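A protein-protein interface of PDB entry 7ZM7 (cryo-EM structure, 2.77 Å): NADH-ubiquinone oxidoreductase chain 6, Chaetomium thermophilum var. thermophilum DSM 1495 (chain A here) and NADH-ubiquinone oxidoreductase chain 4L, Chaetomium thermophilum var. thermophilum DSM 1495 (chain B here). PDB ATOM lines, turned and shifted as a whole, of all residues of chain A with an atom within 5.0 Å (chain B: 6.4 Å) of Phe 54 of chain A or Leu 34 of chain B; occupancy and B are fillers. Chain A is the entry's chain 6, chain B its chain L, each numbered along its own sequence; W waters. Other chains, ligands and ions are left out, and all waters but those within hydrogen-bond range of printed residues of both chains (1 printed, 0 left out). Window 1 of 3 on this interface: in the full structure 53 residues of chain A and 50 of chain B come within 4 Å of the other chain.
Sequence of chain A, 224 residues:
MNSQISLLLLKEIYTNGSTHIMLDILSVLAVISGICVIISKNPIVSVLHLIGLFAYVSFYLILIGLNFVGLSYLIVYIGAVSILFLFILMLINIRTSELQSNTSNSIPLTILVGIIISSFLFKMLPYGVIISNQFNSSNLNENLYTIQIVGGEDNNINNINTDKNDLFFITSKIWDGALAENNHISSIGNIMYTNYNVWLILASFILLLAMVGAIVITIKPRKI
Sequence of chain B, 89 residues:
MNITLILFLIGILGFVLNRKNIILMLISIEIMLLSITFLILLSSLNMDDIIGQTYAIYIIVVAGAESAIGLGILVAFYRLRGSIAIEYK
The side-chain hydroxyl (OH) of Tyr 73 of chain A sits close to the side-chain hydroxyl (OG1) of Thr 37 of chain B (2.2 Å).
The backbone carbonyl oxygen of Leu 7 of chain B sits close to the side-chain hydroxyl of Ser 35 of chain B, at 3.2 Å. The backbone carbonyl oxygen (O) of Ile 31 of chain B is in hydrogen-bond range of the side-chain hydroxyl (OG) of Ser 35 of chain B. The backbone carbonyl oxygen (O) of Phe 54 of chain A sits at hydrogen-bond distance from the side-chain hydroxyl (OG) of Ser 58 of chain A (2.7 Å).
Among the printed residues, merely in contact across the chains: Tyr 77 of chain A with Glu 30 of chain B, Val 57 of chain A with Phe 38 of chain B, Leu 50 of chain A with Ile 31 of chain B, Phe 54 of chain A with Leu 34 of chain B, Leu 53 of chain A with Leu 7 of chain B, Leu 53 of chain A with Leu 34 of chain B, Tyr 73 of chain A with Leu 34 of chain B and Val 57 of chain A with Leu 34 of chain B.
Phe 54 of chain A touches one residue of chain B. Leu 34 of chain B touches just these residues of chain A: Leu 53 (3.8 Å), Phe 54 (3.7 Å), Val 57 (3.9 Å) and Tyr 73 (3.8 Å). Of the printed residues of chain B, Leu 50 of chain A touches Ile 31 (3.6 Å). Printed residues of chain A within 4 Å of Phe 38 of chain B: Val 57 (3.6 Å). Of the printed residues of chain B, Tyr 77 of chain A touches Glu 30. Printed residues of chain A within 4 Å of Leu 7 of chain B: Leu 53 (3.7 Å). Of the printed residues of chain A, Ile 31 of chain B touches Leu 50 (3.6 Å). The nearest residue of chain B that does not touch Phe 54 of chain A is Glu 30 of chain B (4.2 Å). The nearest printed residue of chain A that does not touch Leu 34 of chain B is Tyr 77 of chain A (5.7 Å).
Printed residues of chain A that touch a printed residue of chain B: Leu 50, Leu 53, Phe 54, Val 57, Tyr 73 and Tyr 77.
Water W1 bridges O of Glu 30 of chain B (2.9 Å) and OH of Tyr 77 of chain A (3.4 Å).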
ATOM      1  N   LEU A  50     -21.486  -2.496  11.656  1.00  0.00           N
ATOM      2  CA  LEU A  50     -22.514  -2.052  10.729  1.00  0.00           C
ATOM      3  C   LEU A  50     -22.834  -0.579  10.920  1.00  0.00           C
ATOM      4  O   LEU A  50     -23.035   0.147   9.943  1.00  0.00           O
ATOM      5  CB  LEU A  50     -23.776  -2.887  10.892  1.00  0.00           C
ATOM      6  CG  LEU A  50     -24.545  -2.984   9.586  1.00  0.00           C
ATOM      7  CD1 LEU A  50     -23.738  -3.765   8.576  1.00  0.00           C
ATOM      8  CD2 LEU A  50     -25.901  -3.607   9.793  1.00  0.00           C
ATOM      9  N   ILE A  51     -22.909  -0.121  12.167  1.00  0.00           N
ATOM     10  CA  ILE A  51     -23.138   1.299  12.396  1.00  0.00           C
ATOM     11  C   ILE A  51     -22.003   2.108  11.795  1.00  0.00           C
ATOM     12  O   ILE A  51     -22.208   3.225  11.308  1.00  0.00           O
ATOM     13  CB  ILE A  51     -23.320   1.593  13.898  1.00  0.00           C
ATOM     14  CG1 ILE A  51     -24.435   0.742  14.477  1.00  0.00           C
ATOM     15  CG2 ILE A  51     -23.687   3.035  14.119  1.00  0.00           C
ATOM     16  CD1 ILE A  51     -24.316   0.522  15.942  1.00  0.00           C
ATOM     17  N   GLY A  52     -20.787   1.561  11.820  1.00  0.00           N
ATOM     18  CA  GLY A  52     -19.672   2.229  11.171  1.00  0.00           C
ATOM     19  C   GLY A  52     -19.818   2.299   9.663  1.00  0.00           C
ATOM     20  O   GLY A  52     -19.643   3.358   9.069  1.00  0.00           O
ATOM     21  N   LEU A  53     -20.193   1.183   9.037  1.00  0.00           N
ATOM     22  CA  LEU A  53     -20.358   1.153   7.588  1.00  0.00           C
ATOM     23  C   LEU A  53     -21.440   2.120   7.125  1.00  0.00           C
ATOM     24  O   LEU A  53     -21.269   2.808   6.118  1.00  0.00           O
ATOM     25  CB  LEU A  53     -20.672  -0.274   7.125  1.00  0.00           C
ATOM     26  CG  LEU A  53     -21.124  -0.508   5.674  1.00  0.00           C
ATOM     27  CD1 LEU A  53     -20.177   0.123   4.676  1.00  0.00           C
ATOM     28  CD2 LEU A  53     -21.259  -1.981   5.386  1.00  0.00           C
ATOM     29  N   PHE A  54     -22.560   2.180   7.837  1.00  0.00           N
ATOM     30  CA  PHE A  54     -23.622   3.100   7.453  1.00  0.00           C
ATOM     31  C   PHE A  54     -23.158   4.543   7.540  1.00  0.00           C
ATOM     32  O   PHE A  54     -23.584   5.383   6.741  1.00  0.00           O
ATOM     33  CB  PHE A  54     -24.856   2.885   8.329  1.00  0.00           C
ATOM     34  CG  PHE A  54     -25.631   1.663   7.970  1.00  0.00           C
ATOM     35  CD1 PHE A  54     -25.945   1.397   6.657  1.00  0.00           C
ATOM     36  CD2 PHE A  54     -26.021   0.762   8.935  1.00  0.00           C
ATOM     37  CE1 PHE A  54     -26.638   0.267   6.316  1.00  0.00           C
ATOM     38  CE2 PHE A  54     -26.719  -0.362   8.592  1.00  0.00           C
ATOM     39  CZ  PHE A  54     -27.025  -0.610   7.274  1.00  0.00           C
ATOM     40  N   ALA A  55     -22.292   4.853   8.506  1.00  0.00           N
ATOM     41  CA  ALA A  55     -21.753   6.201   8.618  1.00  0.00           C
ATOM     42  C   ALA A  55     -20.836   6.540   7.453  1.00  0.00           C
ATOM     43  O   ALA A  55     -20.920   7.638   6.899  1.00  0.00           O
ATOM     44  CB  ALA A  55     -21.010   6.360   9.941  1.00  0.00           C
ATOM     45  N   TYR A  56     -19.954   5.619   7.063  1.00  0.00           N
ATOM     46  CA  TYR A  56     -19.016   5.927   5.991  1.00  0.00           C
ATOM     47  C   TYR A  56     -19.739   6.134   4.672  1.00  0.00           C
ATOM     48  O   TYR A  56     -19.375   7.019   3.894  1.00  0.00           O
ATOM     49  CB  TYR A  56     -17.967   4.827   5.857  1.00  0.00           C
ATOM     50  CG  TYR A  56     -17.236   4.593   7.141  1.00  0.00           C
ATOM     51  CD1 TYR A  56     -16.732   5.653   7.868  1.00  0.00           C
ATOM     52  CD2 TYR A  56     -17.053   3.323   7.634  1.00  0.00           C
ATOM     53  CE1 TYR A  56     -16.089   5.463   9.033  1.00  0.00           C
ATOM     54  CE2 TYR A  56     -16.398   3.129   8.813  1.00  0.00           C
ATOM     55  CZ  TYR A  56     -15.920   4.209   9.510  1.00  0.00           C
ATOM     56  OH  TYR A  56     -15.257   4.019  10.691  1.00  0.00           O
ATOM     57  N   VAL A  57     -20.754   5.318   4.403  1.00  0.00           N
ATOM     58  CA  VAL A  57     -21.545   5.476   3.193  1.00  0.00           C
ATOM     59  C   VAL A  57     -22.349   6.765   3.254  1.00  0.00           C
ATOM     60  O   VAL A  57     -22.516   7.458   2.246  1.00  0.00           O
ATOM     61  CB  VAL A  57     -22.440   4.239   2.997  1.00  0.00           C
ATOM     62  CG1 VAL A  57     -23.384   4.428   1.831  1.00  0.00           C
ATOM     63  CG2 VAL A  57     -21.579   3.004   2.805  1.00  0.00           C
ATOM     64  N   SER A  58     -22.856   7.109   4.438  1.00  0.00           N
ATOM     65  CA  SER A  58     -23.581   8.360   4.596  1.00  0.00           C
ATOM     66  C   SER A  58     -22.694   9.548   4.277  1.00  0.00           C
ATOM     67  O   SER A  58     -23.108  10.464   3.564  1.00  0.00           O
ATOM     68  CB  SER A  58     -24.123   8.469   6.012  1.00  0.00           C
ATOM     69  OG  SER A  58     -25.174   7.553   6.219  1.00  0.00           O
ATOM     70  N   TYR A  73     -30.186   8.502   5.617  1.00  0.00           N
ATOM     71  CA  TYR A  73     -29.534   7.269   6.037  1.00  0.00           C
ATOM     72  C   TYR A  73     -29.087   7.364   7.477  1.00  0.00           C
ATOM     73  O   TYR A  73     -29.205   6.401   8.239  1.00  0.00           O
ATOM     74  CB  TYR A  73     -28.318   6.981   5.164  1.00  0.00           C
ATOM     75  CG  TYR A  73     -28.579   6.277   3.870  1.00  0.00           C
ATOM     76  CD1 TYR A  73     -28.811   4.912   3.834  1.00  0.00           C
ATOM     77  CD2 TYR A  73     -28.535   6.963   2.685  1.00  0.00           C
ATOM     78  CE1 TYR A  73     -29.020   4.269   2.658  1.00  0.00           C
ATOM     79  CE2 TYR A  73     -28.743   6.337   1.502  1.00  0.00           C
ATOM     80  CZ  TYR A  73     -28.983   4.993   1.487  1.00  0.00           C
ATOM     81  OH  TYR A  73     -29.195   4.398   0.277  1.00  0.00           O
ATOM     82  N   LEU A  74     -28.530   8.509   7.855  1.00  0.00           N
ATOM     83  CA  LEU A  74     -28.107   8.717   9.229  1.00  0.00           C
ATOM     84  C   LEU A  74     -29.290   8.625  10.180  1.00  0.00           C
ATOM     85  O   LEU A  74     -29.251   7.883  11.166  1.00  0.00           O
ATOM     86  CB  LEU A  74     -27.416  10.070   9.348  1.00  0.00           C
ATOM     87  CG  LEU A  74     -25.933  10.096   9.044  1.00  0.00           C
ATOM     88  CD1 LEU A  74     -25.342  11.406   9.510  1.00  0.00           C
ATOM     89  CD2 LEU A  74     -25.236   8.933   9.716  1.00  0.00           C
ATOM     90  N   TYR A  77     -31.007   4.592   9.558  1.00  0.00           N
ATOM     91  CA  TYR A  77     -30.260   3.348   9.882  1.00  0.00           C
ATOM     92  C   TYR A  77     -29.575   3.451  11.234  1.00  0.00           C
ATOM     93  O   TYR A  77     -29.924   2.690  12.146  1.00  0.00           O
ATOM     94  CB  TYR A  77     -29.297   2.965   8.760  1.00  0.00           C
ATOM     95  CG  TYR A  77     -30.074   2.388   7.614  1.00  0.00           C
ATOM     96  CD1 TYR A  77     -30.658   1.140   7.730  1.00  0.00           C
ATOM     97  CD2 TYR A  77     -30.322   3.131   6.476  1.00  0.00           C
ATOM     98  CE1 TYR A  77     -31.425   0.612   6.710  1.00  0.00           C
ATOM     99  CE2 TYR A  77     -31.081   2.616   5.444  1.00  0.00           C
ATOM    100  CZ  TYR A  77     -31.634   1.357   5.567  1.00  0.00           C
ATOM    101  OH  TYR A  77     -32.390   0.850   4.561  1.00  0.00           O
ATOM    102  N   ILE A  78     -28.621   4.367  11.338  1.00  0.00           N
ATOM    103  CA  ILE A  78     -27.923   4.533  12.602  1.00  0.00           C
ATOM    104  C   ILE A  78     -28.883   5.022  13.664  1.00  0.00           C
ATOM    105  O   ILE A  78     -28.777   4.652  14.834  1.00  0.00           O
ATOM    106  CB  ILE A  78     -26.734   5.488  12.426  1.00  0.00           C
ATOM    107  CG1 ILE A  78     -25.732   4.909  11.441  1.00  0.00           C
ATOM    108  CG2 ILE A  78     -26.075   5.791  13.759  1.00  0.00           C
ATOM    109  CD1 ILE A  78     -24.513   5.728  11.320  1.00  0.00           C
ATOM    110  N   THR B   4     -19.667  -0.188  -4.781  1.00  0.00           N
ATOM    111  CA  THR B   4     -20.994  -0.780  -4.643  1.00  0.00           C
ATOM    112  C   THR B   4     -20.942  -2.284  -4.824  1.00  0.00           C
ATOM    113  O   THR B   4     -21.613  -3.025  -4.103  1.00  0.00           O
ATOM    114  CB  THR B   4     -21.971  -0.145  -5.636  1.00  0.00           C
ATOM    115  OG1 THR B   4     -21.478  -0.279  -6.969  1.00  0.00           O
ATOM    116  CG2 THR B   4     -22.140   1.302  -5.333  1.00  0.00           C
ATOM    117  N   LEU B   7     -19.207  -4.025  -1.758  1.00  0.00           N
ATOM    118  CA  LEU B   7     -20.050  -4.075  -0.579  1.00  0.00           C
ATOM    119  C   LEU B   7     -21.177  -5.076  -0.782  1.00  0.00           C
ATOM    120  O   LEU B   7     -21.718  -5.614   0.188  1.00  0.00           O
ATOM    121  CB  LEU B   7     -20.552  -2.661  -0.281  1.00  0.00           C
ATOM    122  CG  LEU B   7     -21.163  -2.202   1.044  1.00  0.00           C
ATOM    123  CD1 LEU B   7     -20.990  -0.696   1.135  1.00  0.00           C
ATOM    124  CD2 LEU B   7     -22.604  -2.529   1.203  1.00  0.00           C
ATOM    125  N   ILE B  29     -28.304  -9.226   4.714  1.00  0.00           N
ATOM    126  CA  ILE B  29     -29.417  -8.795   3.827  1.00  0.00           C
ATOM    127  C   ILE B  29     -29.414  -7.270   3.771  1.00  0.00           C
ATOM    128  O   ILE B  29     -29.633  -6.712   2.680  1.00  0.00           O
ATOM    129  CB  ILE B  29     -30.761  -9.368   4.317  1.00  0.00           C
ATOM    130  CG1 ILE B  29     -30.878 -10.866   4.029  1.00  0.00           C
ATOM    131  CG2 ILE B  29     -31.941  -8.597   3.741  1.00  0.00           C
ATOM    132  CD1 ILE B  29     -32.074 -11.523   4.677  1.00  0.00           C
ATOM    133  N   GLU B  30     -29.095  -6.624   4.886  1.00  0.00           N
ATOM    134  CA  GLU B  30     -29.135  -5.149   4.946  1.00  0.00           C
ATOM    135  C   GLU B  30     -27.860  -4.591   4.326  1.00  0.00           C
ATOM    136  O   GLU B  30     -27.931  -3.501   3.748  1.00  0.00           O
ATOM    137  CB  GLU B  30     -29.251  -4.728   6.405  1.00  0.00           C
ATOM    138  CG  GLU B  30     -30.677  -4.447   6.830  1.00  0.00           C
ATOM    139  CD  GLU B  30     -30.790  -3.331   7.853  1.00  0.00           C
ATOM    140  OE1 GLU B  30     -29.930  -3.269   8.751  1.00  0.00           O
ATOM    141  OE2 GLU B  30     -31.728  -2.519   7.736  1.00  0.00           O
ATOM    142  N   ILE B  31     -26.738  -5.296   4.430  1.00  0.00           N
ATOM    143  CA  ILE B  31     -25.556  -4.843   3.701  1.00  0.00           C
ATOM    144  C   ILE B  31     -25.809  -4.901   2.202  1.00  0.00           C
ATOM    145  O   ILE B  31     -25.379  -4.018   1.456  1.00  0.00           O
ATOM    146  CB  ILE B  31     -24.310  -5.666   4.087  1.00  0.00           C
ATOM    147  CG1 ILE B  31     -24.130  -5.737   5.595  1.00  0.00           C
ATOM    148  CG2 ILE B  31     -23.074  -5.042   3.534  1.00  0.00           C
ATOM    149  CD1 ILE B  31     -23.076  -6.701   6.013  1.00  0.00           C
ATOM    150  N   MET B  32     -26.503  -5.941   1.734  1.00  0.00           N
ATOM    151  CA  MET B  32     -26.845  -6.115   0.295  1.00  0.00           C
ATOM    152  C   MET B  32     -27.785  -4.988  -0.152  1.00  0.00           C
ATOM    153  O   MET B  32     -27.593  -4.480  -1.262  1.00  0.00           O
ATOM    154  CB  MET B  32     -27.424  -7.501  -0.010  1.00  0.00           C
ATOM    155  CG  MET B  32     -26.445  -8.629   0.190  1.00  0.00           C
ATOM    156  SD  MET B  32     -27.275 -10.234   0.237  1.00  0.00           S
ATOM    157  CE  MET B  32     -27.742 -10.410  -1.483  1.00  0.00           C
ATOM    158  N   LEU B  33     -28.759  -4.627   0.681  1.00  0.00           N
ATOM    159  CA  LEU B  33     -29.691  -3.506   0.382  1.00  0.00           C
ATOM    160  C   LEU B  33     -28.920  -2.190   0.311  1.00  0.00           C
ATOM    161  O   LEU B  33     -29.264  -1.402  -0.564  1.00  0.00           O
ATOM    162  CB  LEU B  33     -30.815  -3.476   1.416  1.00  0.00           C
ATOM    163  CG  LEU B  33     -31.662  -4.745   1.494  1.00  0.00           C
ATOM    164  CD1 LEU B  33     -32.646  -4.683   2.649  1.00  0.00           C
ATOM    165  CD2 LEU B  33     -32.391  -4.998   0.187  1.00  0.00           C
ATOM    166  N   LEU B  34     -27.867  -2.018   1.122  1.00  0.00           N
ATOM    167  CA  LEU B  34     -27.098  -0.751   1.153  1.00  0.00           C
ATOM    168  C   LEU B  34     -26.210  -0.732  -0.077  1.00  0.00           C
ATOM    169  O   LEU B  34     -25.870   0.340  -0.530  1.00  0.00           O
ATOM    170  CB  LEU B  34     -26.252  -0.667   2.428  1.00  0.00           C
ATOM    171  CG  LEU B  34     -25.316   0.532   2.538  1.00  0.00           C
ATOM    172  CD1 LEU B  34     -26.093   1.787   2.896  1.00  0.00           C
ATOM    173  CD2 LEU B  34     -24.223   0.267   3.556  1.00  0.00           C
ATOM    174  N   SER B  35     -25.897  -1.891  -0.632  1.00  0.00           N
ATOM    175  CA  SER B  35     -25.165  -1.818  -1.886  1.00  0.00           C
ATOM    176  C   SER B  35     -26.062  -1.338  -3.008  1.00  0.00           C
ATOM    177  O   SER B  35     -25.686  -0.464  -3.790  1.00  0.00           O
ATOM    178  CB  SER B  35     -24.605  -3.189  -2.244  1.00  0.00           C
ATOM    179  OG  SER B  35     -23.865  -3.705  -1.193  1.00  0.00           O
ATOM    180  N   ILE B  36     -27.238  -1.944  -3.130  1.00  0.00           N
ATOM    181  CA  ILE B  36     -28.109  -1.679  -4.264  1.00  0.00           C
ATOM    182  C   ILE B  36     -28.647  -0.259  -4.201  1.00  0.00           C
ATOM    183  O   ILE B  36     -28.710   0.432  -5.219  1.00  0.00           O
ATOM    184  CB  ILE B  36     -29.228  -2.740  -4.325  1.00  0.00           C
ATOM    185  CG1 ILE B  36     -28.676  -4.048  -4.883  1.00  0.00           C
ATOM    186  CG2 ILE B  36     -30.390  -2.265  -5.164  1.00  0.00           C
ATOM    187  CD1 ILE B  36     -29.316  -5.270  -4.317  1.00  0.00           C
ATOM    188  N   THR B  37     -29.015   0.210  -3.011  1.00  0.00           N
ATOM    189  CA  THR B  37     -29.419   1.604  -2.881  1.00  0.00           C
ATOM    190  C   THR B  37     -28.270   2.539  -3.220  1.00  0.00           C
ATOM    191  O   THR B  37     -28.463   3.550  -3.899  1.00  0.00           O
ATOM    192  CB  THR B  37     -29.948   1.888  -1.471  1.00  0.00           C
ATOM    193  OG1 THR B  37     -30.254   3.279  -1.343  1.00  0.00           O
ATOM    194  CG2 THR B  37     -28.939   1.558  -0.438  1.00  0.00           C
ATOM    195  N   PHE B  38     -27.067   2.200  -2.779  1.00  0.00           N
ATOM    196  CA  PHE B  38     -25.907   3.032  -3.034  1.00  0.00           C
ATOM    197  C   PHE B  38     -25.558   3.078  -4.515  1.00  0.00           C
ATOM    198  O   PHE B  38     -25.144   4.125  -5.026  1.00  0.00           O
ATOM    199  CB  PHE B  38     -24.753   2.514  -2.198  1.00  0.00           C
ATOM    200  CG  PHE B  38     -23.625   3.454  -2.090  1.00  0.00           C
ATOM    201  CD1 PHE B  38     -23.827   4.755  -1.699  1.00  0.00           C
ATOM    202  CD2 PHE B  38     -22.359   3.060  -2.447  1.00  0.00           C
ATOM    203  CE1 PHE B  38     -22.777   5.619  -1.627  1.00  0.00           C
ATOM    204  CE2 PHE B  38     -21.326   3.926  -2.370  1.00  0.00           C
ATOM    205  CZ  PHE B  38     -21.541   5.191  -1.968  1.00  0.00           C
ATOM    206  N   LEU B  39     -25.714   1.957  -5.224  1.00  0.00           N
ATOM    207  CA  LEU B  39     -25.480   1.957  -6.661  1.00  0.00           C
ATOM    208  C   LEU B  39     -26.517   2.802  -7.393  1.00  0.00           C
ATOM    209  O   LEU B  39     -26.167   3.589  -8.276  1.00  0.00           O
ATOM    210  CB  LEU B  39     -25.471   0.526  -7.191  1.00  0.00           C
ATOM    211  CG  LEU B  39     -25.678   0.337  -8.694  1.00  0.00           C
ATOM    212  CD1 LEU B  39     -24.518   0.878  -9.469  1.00  0.00           C
ATOM    213  CD2 LEU B  39     -25.909  -1.106  -9.056  1.00  0.00           C
HETATM  214  O   HOH W   1     -30.076  -1.700   4.443  1.00  0.00           O
